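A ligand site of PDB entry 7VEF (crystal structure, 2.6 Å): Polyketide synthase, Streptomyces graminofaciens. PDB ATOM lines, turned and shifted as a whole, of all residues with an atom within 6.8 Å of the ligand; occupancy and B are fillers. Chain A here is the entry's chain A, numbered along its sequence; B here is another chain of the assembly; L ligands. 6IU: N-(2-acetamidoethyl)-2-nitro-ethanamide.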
ATOM      1  N   GLN A 191     -20.619  10.344 -30.707  1.00  0.00           N
ATOM      2  CA  GLN A 191     -19.862  11.419 -30.016  1.00  0.00           C
ATOM      3  C   GLN A 191     -18.605  11.794 -30.809  1.00  0.00           C
ATOM      4  O   GLN A 191     -17.830  12.611 -30.277  1.00  0.00           O
ATOM      5  CB  GLN A 191     -19.516  11.006 -28.587  1.00  0.00           C
ATOM      6  CG  GLN A 191     -20.737  10.720 -27.731  1.00  0.00           C
ATOM      7  CD  GLN A 191     -21.239   9.310 -27.862  1.00  0.00           C
ATOM      8  OE1 GLN A 191     -20.827   8.560 -28.744  1.00  0.00           O
ATOM      9  NE2 GLN A 191     -22.151   8.929 -26.977  1.00  0.00           N
ATOM     10  N   SER A 192     -18.414  11.253 -32.019  1.00  0.00           N
ATOM     11  CA  SER A 192     -17.316  11.623 -32.956  1.00  0.00           C
ATOM     12  C   SER A 192     -17.868  12.227 -34.261  1.00  0.00           C
ATOM     13  O   SER A 192     -17.058  12.580 -35.132  1.00  0.00           O
ATOM     14  CB  SER A 192     -16.419  10.433 -33.240  1.00  0.00           C
ATOM     15  OG  SER A 192     -17.140   9.334 -33.747  1.00  0.00           O
ATOM     16  N   PHE A 233     -27.418   5.048 -18.737  1.00  0.00           N
ATOM     17  CA  PHE A 233     -26.195   4.439 -19.322  1.00  0.00           C
ATOM     18  C   PHE A 233     -25.093   4.330 -18.252  1.00  0.00           C
ATOM     19  O   PHE A 233     -24.353   3.348 -18.262  1.00  0.00           O
ATOM     20  CB  PHE A 233     -25.737   5.284 -20.514  1.00  0.00           C
ATOM     21  CG  PHE A 233     -24.778   4.606 -21.467  1.00  0.00           C
ATOM     22  CD1 PHE A 233     -25.061   3.361 -22.007  1.00  0.00           C
ATOM     23  CD2 PHE A 233     -23.624   5.255 -21.862  1.00  0.00           C
ATOM     24  CE1 PHE A 233     -24.181   2.763 -22.898  1.00  0.00           C
ATOM     25  CE2 PHE A 233     -22.743   4.667 -22.753  1.00  0.00           C
ATOM     26  CZ  PHE A 233     -23.028   3.421 -23.279  1.00  0.00           C
ATOM     27  N   GLY A 234     -25.005   5.302 -17.337  1.00  0.00           N
ATOM     28  CA  GLY A 234     -24.002   5.365 -16.249  1.00  0.00           C
ATOM     29  C   GLY A 234     -22.835   6.293 -16.595  1.00  0.00           C
ATOM     30  O   GLY A 234     -21.907   6.402 -15.775  1.00  0.00           O
ATOM     31  N   GLY A 235     -22.893   6.976 -17.743  1.00  0.00           N
ATOM     32  CA  GLY A 235     -21.785   7.807 -18.235  1.00  0.00           C
ATOM     33  C   GLY A 235     -21.614   9.131 -17.510  1.00  0.00           C
ATOM     34  O   GLY A 235     -20.561   9.768 -17.741  1.00  0.00           O
ATOM     35  N   PHE A 252     -18.761  12.164 -17.465  1.00  0.00           N
ATOM     36  CA  PHE A 252     -18.796  13.459 -18.199  1.00  0.00           C
ATOM     37  C   PHE A 252     -20.027  14.251 -17.776  1.00  0.00           C
ATOM     38  O   PHE A 252     -20.999  13.657 -17.254  1.00  0.00           O
ATOM     39  CB  PHE A 252     -18.797  13.258 -19.717  1.00  0.00           C
ATOM     40  CG  PHE A 252     -19.939  12.457 -20.287  1.00  0.00           C
ATOM     41  CD1 PHE A 252     -19.876  11.067 -20.365  1.00  0.00           C
ATOM     42  CD2 PHE A 252     -21.069  13.085 -20.795  1.00  0.00           C
ATOM     43  CE1 PHE A 252     -20.928  10.334 -20.899  1.00  0.00           C
ATOM     44  CE2 PHE A 252     -22.107  12.352 -21.327  1.00  0.00           C
ATOM     45  CZ  PHE A 252     -22.047  10.982 -21.377  1.00  0.00           C
ATOM     46  N   THR A 293     -16.294  -4.560 -24.426  1.00  0.00           N
ATOM     47  CA  THR A 293     -17.745  -4.254 -24.529  1.00  0.00           C
ATOM     48  C   THR A 293     -17.930  -3.466 -25.828  1.00  0.00           C
ATOM     49  O   THR A 293     -16.937  -2.923 -26.306  1.00  0.00           O
ATOM     50  CB  THR A 293     -18.220  -3.459 -23.298  1.00  0.00           C
ATOM     51  OG1 THR A 293     -18.141  -4.342 -22.172  1.00  0.00           O
ATOM     52  CG2 THR A 293     -19.629  -2.915 -23.362  1.00  0.00           C
ATOM     53  N   THR A 295     -19.144  -0.621 -26.055  1.00  0.00           N
ATOM     54  CA  THR A 295     -19.036   0.810 -25.666  1.00  0.00           C
ATOM     55  C   THR A 295     -17.645   1.127 -25.111  1.00  0.00           C
ATOM     56  O   THR A 295     -17.295   2.310 -25.048  1.00  0.00           O
ATOM     57  CB  THR A 295     -20.156   1.190 -24.677  1.00  0.00           C
ATOM     58  OG1 THR A 295     -20.095   0.367 -23.510  1.00  0.00           O
ATOM     59  CG2 THR A 295     -21.535   1.024 -25.298  1.00  0.00           C
ATOM     60  N   THR A 296     -16.867   0.117 -24.738  1.00  0.00           N
ATOM     61  CA  THR A 296     -15.452   0.276 -24.318  1.00  0.00           C
ATOM     62  C   THR A 296     -14.627   0.705 -25.536  1.00  0.00           C
ATOM     63  O   THR A 296     -14.768   0.148 -26.623  1.00  0.00           O
ATOM     64  CB  THR A 296     -14.903  -1.006 -23.682  1.00  0.00           C
ATOM     65  OG1 THR A 296     -15.845  -1.449 -22.703  1.00  0.00           O
ATOM     66  CG2 THR A 296     -13.548  -0.790 -23.042  1.00  0.00           C
ATOM     67  N   PRO A 297     -13.790   1.759 -25.406  1.00  0.00           N
ATOM     68  CA  PRO A 297     -12.808   2.093 -26.431  1.00  0.00           C
ATOM     69  C   PRO A 297     -11.628   1.112 -26.372  1.00  0.00           C
ATOM     70  O   PRO A 297     -11.404   0.518 -25.320  1.00  0.00           O
ATOM     71  CB  PRO A 297     -12.418   3.541 -26.116  1.00  0.00           C
ATOM     72  CG  PRO A 297     -12.656   3.687 -24.633  1.00  0.00           C
ATOM     73  CD  PRO A 297     -13.768   2.718 -24.279  1.00  0.00           C
ATOM     74  N   HIS A 326     -10.255  13.938 -26.613  1.00  0.00           N
ATOM     75  CA  HIS A 326     -11.675  13.616 -26.321  1.00  0.00           C
ATOM     76  C   HIS A 326     -11.904  13.901 -24.827  1.00  0.00           C
ATOM     77  O   HIS A 326     -12.675  14.818 -24.508  1.00  0.00           O
ATOM     78  CB  HIS A 326     -11.966  12.188 -26.772  1.00  0.00           C
ATOM     79  CG  HIS A 326     -13.414  11.863 -26.835  1.00  0.00           C
ATOM     80  ND1 HIS A 326     -14.278  12.553 -27.640  1.00  0.00           N
ATOM     81  CD2 HIS A 326     -14.145  10.933 -26.191  1.00  0.00           C
ATOM     82  CE1 HIS A 326     -15.495  12.060 -27.494  1.00  0.00           C
ATOM     83  NE2 HIS A 326     -15.435  11.072 -26.594  1.00  0.00           N
ATOM     84  N   GLY A 327     -11.193  13.193 -23.944  1.00  0.00           N
ATOM     85  CA  GLY A 327     -11.095  13.484 -22.497  1.00  0.00           C
ATOM     86  C   GLY A 327     -12.450  13.754 -21.872  1.00  0.00           C
ATOM     87  O   GLY A 327     -12.668  14.858 -21.349  1.00  0.00           O
ATOM     88  N   THR A 328     -13.341  12.759 -21.923  1.00  0.00           N
ATOM     89  CA  THR A 328     -14.722  12.832 -21.398  1.00  0.00           C
ATOM     90  C   THR A 328     -14.689  12.913 -19.870  1.00  0.00           C
ATOM     91  O   THR A 328     -15.603  13.527 -19.291  1.00  0.00           O
ATOM     92  CB  THR A 328     -15.530  11.635 -21.905  1.00  0.00           C
ATOM     93  OG1 THR A 328     -14.809  10.428 -21.658  1.00  0.00           O
ATOM     94  CG2 THR A 328     -15.830  11.728 -23.390  1.00  0.00           C
ATOM     95  N   GLY A 329     -13.658  12.314 -19.261  1.00  0.00           N
ATOM     96  CA  GLY A 329     -13.506  12.204 -17.791  1.00  0.00           C
ATOM     97  C   GLY A 329     -14.141  10.924 -17.267  1.00  0.00           C
ATOM     98  O   GLY A 329     -14.492  10.887 -16.068  1.00  0.00           O
ATOM     99  N   THR A 330     -14.296   9.912 -18.120  1.00  0.00           N
ATOM    100  CA  THR A 330     -14.796   8.553 -17.750  1.00  0.00           C
ATOM    101  C   THR A 330     -13.638   7.723 -17.170  1.00  0.00           C
ATOM    102  O   THR A 330     -12.514   7.815 -17.722  1.00  0.00           O
ATOM    103  CB  THR A 330     -15.471   7.887 -18.965  1.00  0.00           C
ATOM    104  OG1 THR A 330     -14.679   8.026 -20.143  1.00  0.00           O
ATOM    105  CG2 THR A 330     -16.838   8.474 -19.223  1.00  0.00           C
ATOM    106  N   LYS A 331     -13.904   6.957 -16.106  1.00  0.00           N
ATOM    107  CA  LYS A 331     -12.911   6.077 -15.428  1.00  0.00           C
ATOM    108  C   LYS A 331     -12.218   5.165 -16.451  1.00  0.00           C
ATOM    109  O   LYS A 331     -10.977   5.074 -16.397  1.00  0.00           O
ATOM    110  CB  LYS A 331     -13.563   5.227 -14.328  1.00  0.00           C
ATOM    111  CG  LYS A 331     -13.880   5.998 -13.053  1.00  0.00           C
ATOM    112  CD  LYS A 331     -14.625   5.210 -11.994  1.00  0.00           C
ATOM    113  CE  LYS A 331     -15.153   6.098 -10.884  1.00  0.00           C
ATOM    114  NZ  LYS A 331     -15.918   5.322  -9.884  1.00  0.00           N
ATOM    115  N   VAL A 332     -12.996   4.534 -17.338  1.00  0.00           N
ATOM    116  CA  VAL A 332     -12.518   3.546 -18.364  1.00  0.00           C
ATOM    117  C   VAL A 332     -11.772   4.285 -19.488  1.00  0.00           C
ATOM    118  O   VAL A 332     -10.665   3.843 -19.844  1.00  0.00           O
ATOM    119  CB  VAL A 332     -13.666   2.705 -18.943  1.00  0.00           C
ATOM    120  CG1 VAL A 332     -13.322   2.095 -20.282  1.00  0.00           C
ATOM    121  CG2 VAL A 332     -14.126   1.634 -17.969  1.00  0.00           C
ATOM    122  N   GLY A 333     -12.383   5.345 -20.023  1.00  0.00           N
ATOM    123  CA  GLY A 333     -12.049   5.955 -21.329  1.00  0.00           C
ATOM    124  C   GLY A 333     -10.865   6.895 -21.287  1.00  0.00           C
ATOM    125  O   GLY A 333     -10.213   7.034 -22.334  1.00  0.00           O
ATOM    126  N   ASP A 334     -10.597   7.519 -20.131  1.00  0.00           N
ATOM    127  CA  ASP A 334      -9.481   8.467 -19.913  1.00  0.00           C
ATOM    128  C   ASP A 334      -8.143   7.727 -20.026  1.00  0.00           C
ATOM    129  O   ASP A 334      -7.335   8.060 -20.884  1.00  0.00           O
ATOM    130  CB  ASP A 334      -9.641   9.225 -18.594  1.00  0.00           C
ATOM    131  CG  ASP A 334     -10.272  10.607 -18.690  1.00  0.00           C
ATOM    132  OD1 ASP A 334     -10.772  10.976 -19.792  1.00  0.00           O
ATOM    133  OD2 ASP A 334     -10.250  11.337 -17.646  1.00  0.00           O
ATOM    134  N   LYS A 359     -14.128  20.095 -22.979  1.00  0.00           N
ATOM    135  CA  LYS A 359     -15.199  19.437 -22.171  1.00  0.00           C
ATOM    136  C   LYS A 359     -15.089  19.827 -20.692  1.00  0.00           C
ATOM    137  O   LYS A 359     -16.098  19.660 -19.953  1.00  0.00           O
ATOM    138  CB  LYS A 359     -15.171  17.909 -22.328  1.00  0.00           C
ATOM    139  CG  LYS A 359     -15.487  17.400 -23.732  1.00  0.00           C
ATOM    140  CD  LYS A 359     -15.700  15.905 -23.795  1.00  0.00           C
ATOM    141  CE  LYS A 359     -15.960  15.385 -25.191  1.00  0.00           C
ATOM    142  NZ  LYS A 359     -14.882  15.755 -26.138  1.00  0.00           N
ATOM    143  N   HIS A 364     -19.603  17.924 -22.455  1.00  0.00           N
ATOM    144  CA  HIS A 364     -19.499  16.943 -23.564  1.00  0.00           C
ATOM    145  C   HIS A 364     -20.629  17.201 -24.572  1.00  0.00           C
ATOM    146  O   HIS A 364     -21.781  16.844 -24.257  1.00  0.00           O
ATOM    147  CB  HIS A 364     -19.524  15.532 -22.977  1.00  0.00           C
ATOM    148  CG  HIS A 364     -19.212  14.455 -23.957  1.00  0.00           C
ATOM    149  ND1 HIS A 364     -19.023  14.727 -25.290  1.00  0.00           N
ATOM    150  CD2 HIS A 364     -19.108  13.120 -23.814  1.00  0.00           C
ATOM    151  CE1 HIS A 364     -18.790  13.585 -25.926  1.00  0.00           C
ATOM    152  NE2 HIS A 364     -18.842  12.589 -25.043  1.00  0.00           N
ATOM    153  N   GLU A 366     -21.172  15.913 -27.393  1.00  0.00           N
ATOM    154  CA  GLU A 366     -21.559  14.641 -28.055  1.00  0.00           C
ATOM    155  C   GLU A 366     -21.297  14.785 -29.573  1.00  0.00           C
ATOM    156  O   GLU A 366     -20.132  14.904 -29.954  1.00  0.00           O
ATOM    157  CB  GLU A 366     -23.005  14.278 -27.682  1.00  0.00           C
ATOM    158  CG  GLU A 366     -23.274  14.334 -26.191  1.00  0.00           C
ATOM    159  CD  GLU A 366     -23.668  13.037 -25.512  1.00  0.00           C
ATOM    160  OE1 GLU A 366     -24.740  13.012 -24.858  1.00  0.00           O
ATOM    161  OE2 GLU A 366     -22.888  12.056 -25.602  1.00  0.00           O
ATOM    162  N   PHE A 432     -13.977  10.536 -30.217  1.00  0.00           N
ATOM    163  CA  PHE A 432     -14.383   9.112 -30.220  1.00  0.00           C
ATOM    164  C   PHE A 432     -15.893   8.992 -29.967  1.00  0.00           C
ATOM    165  O   PHE A 432     -16.435   9.746 -29.124  1.00  0.00           O
ATOM    166  CB  PHE A 432     -13.582   8.329 -29.182  1.00  0.00           C
ATOM    167  CG  PHE A 432     -12.116   8.675 -29.145  1.00  0.00           C
ATOM    168  CD1 PHE A 432     -11.395   8.845 -30.318  1.00  0.00           C
ATOM    169  CD2 PHE A 432     -11.457   8.831 -27.934  1.00  0.00           C
ATOM    170  CE1 PHE A 432     -10.043   9.172 -30.283  1.00  0.00           C
ATOM    171  CE2 PHE A 432     -10.106   9.158 -27.899  1.00  0.00           C
ATOM    172  CZ  PHE A 432      -9.399   9.319 -29.074  1.00  0.00           C
ATOM    173  N   GLY A 433     -16.536   8.066 -30.688  1.00  0.00           N
ATOM    174  CA  GLY A 433     -17.951   7.686 -30.490  1.00  0.00           C
ATOM    175  C   GLY A 433     -18.052   6.411 -29.654  1.00  0.00           C
ATOM    176  O   GLY A 433     -17.121   5.597 -29.727  1.00  0.00           O
ATOM    177  N   MET A 434     -19.155   6.245 -28.907  1.00  0.00           N
ATOM    178  CA  MET A 434     -19.408   5.062 -28.042  1.00  0.00           C
ATOM    179  C   MET A 434     -19.453   3.789 -28.898  1.00  0.00           C
ATOM    180  O   MET A 434     -19.035   2.723 -28.420  1.00  0.00           O
ATOM    181  CB  MET A 434     -20.730   5.200 -27.271  1.00  0.00           C
ATOM    182  CG  MET A 434     -21.940   5.317 -28.186  1.00  0.00           C
ATOM    183  SD  MET A 434     -23.478   5.726 -27.320  1.00  0.00           S
ATOM    184  CE  MET A 434     -24.278   6.713 -28.590  1.00  0.00           C
ATOM    185  N   GLY A 435     -19.938   3.881 -30.145  1.00  0.00           N
ATOM    186  CA  GLY A 435     -20.009   2.719 -31.053  1.00  0.00           C
ATOM    187  C   GLY A 435     -18.680   2.399 -31.696  1.00  0.00           C
ATOM    188  O   GLY A 435     -18.677   1.596 -32.624  1.00  0.00           O
ATOM    189  N   MET B 162     -29.892   3.589 -24.616  1.00  0.00           N
ATOM    190  CA  MET B 162     -28.830   4.434 -25.236  1.00  0.00           C
ATOM    191  C   MET B 162     -28.298   3.820 -26.542  1.00  0.00           C
ATOM    192  O   MET B 162     -28.389   4.491 -27.565  1.00  0.00           O
ATOM    193  CB  MET B 162     -27.646   4.627 -24.292  1.00  0.00           C
ATOM    194  CG  MET B 162     -26.461   5.320 -24.947  1.00  0.00           C
ATOM    195  SD  MET B 162     -26.625   7.113 -24.955  1.00  0.00           S
ATOM    196  CE  MET B 162     -25.493   7.520 -23.628  1.00  0.00           C
HETATM  197  OAL 6IU L   1     -17.804   9.952 -25.616  1.00  0.00           O
HETATM  198  N   6IU L   1     -17.770   8.360 -25.566  1.00  0.00           N
HETATM  199  OAM 6IU L   1     -19.182   7.741 -25.464  1.00  0.00           O
HETATM  200  CA  6IU L   1     -16.532   7.510 -25.596  1.00  0.00           C
HETATM  201  C   6IU L   1     -15.997   7.173 -24.132  1.00  0.00           C
HETATM  202  O   6IU L   1     -15.189   7.899 -23.540  1.00  0.00           O
HETATM  203  NAG 6IU L   1     -16.478   6.030 -23.570  1.00  0.00           N
HETATM  204  CAF 6IU L   1     -16.138   5.539 -22.215  1.00  0.00           C
HETATM  205  CAE 6IU L   1     -17.446   5.067 -21.524  1.00  0.00           C
HETATM  206  NAD 6IU L   1     -17.446   3.576 -21.520  1.00  0.00           N
HETATM  207  CAB 6IU L   1     -18.256   2.775 -20.763  1.00  0.00           C
HETATM  208  OAC 6IU L   1     -19.124   3.155 -19.988  1.00  0.00           O
HETATM  209  CAA 6IU L   1     -17.982   1.273 -20.928  1.00  0.00           C
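OAL of the ligand lies within hydrogen-bond range of NE2 of His 326 (2.8 Å). OAL of the ligand is in hydrogen-bond range of NE2 of His 364, 2.9 Å away. An oxygen (O) of the ligand lies within hydrogen-bond range of the side-chain hydroxyl of Thr 328, 3.2 Å away. An oxygen (O) of the ligand sits at hydrogen-bond distance from the side-chain hydroxyl (OG1) of Thr 330 (3.4 Å).
A ring nitrogen (NE2) of His 326 lies close to the backbone carbonyl oxygen of Phe 432, 3.0 Å away. O of His 326 sits at hydrogen-bond distance from NZ of Lys 359. A ring nitrogen (ND1) of His 364 lies close to the backbone NH (N) of Glu 366, at 3.2 Å. OG1 of Thr 328 is in hydrogen-bond range of OG1 of Thr 330. The backbone NH (N) of Met 434 lies within hydrogen-bond range of the side-chain amide oxygen (OE1) of Gln 191, 2.9 Å away. NE2 of Gln 191 sits close to OE2 of Glu 366.
Merely in contact with the ligand: Thr 295 (3.5 Å), Met 434 (3.5 Å), Gln 191 (3.5 Å), Phe 432 (3.8 Å) and Thr 296 (3.9 Å). Hydrophobic or aromatic side chains that line the ligand: His 326, His 364 and Met 434. Nine residues have an atom within 4 Å of the ligand: Gln 191, Thr 295, Thr 296, His 326, Thr 328, Thr 330, His 364, Phe 432 and Met 434.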
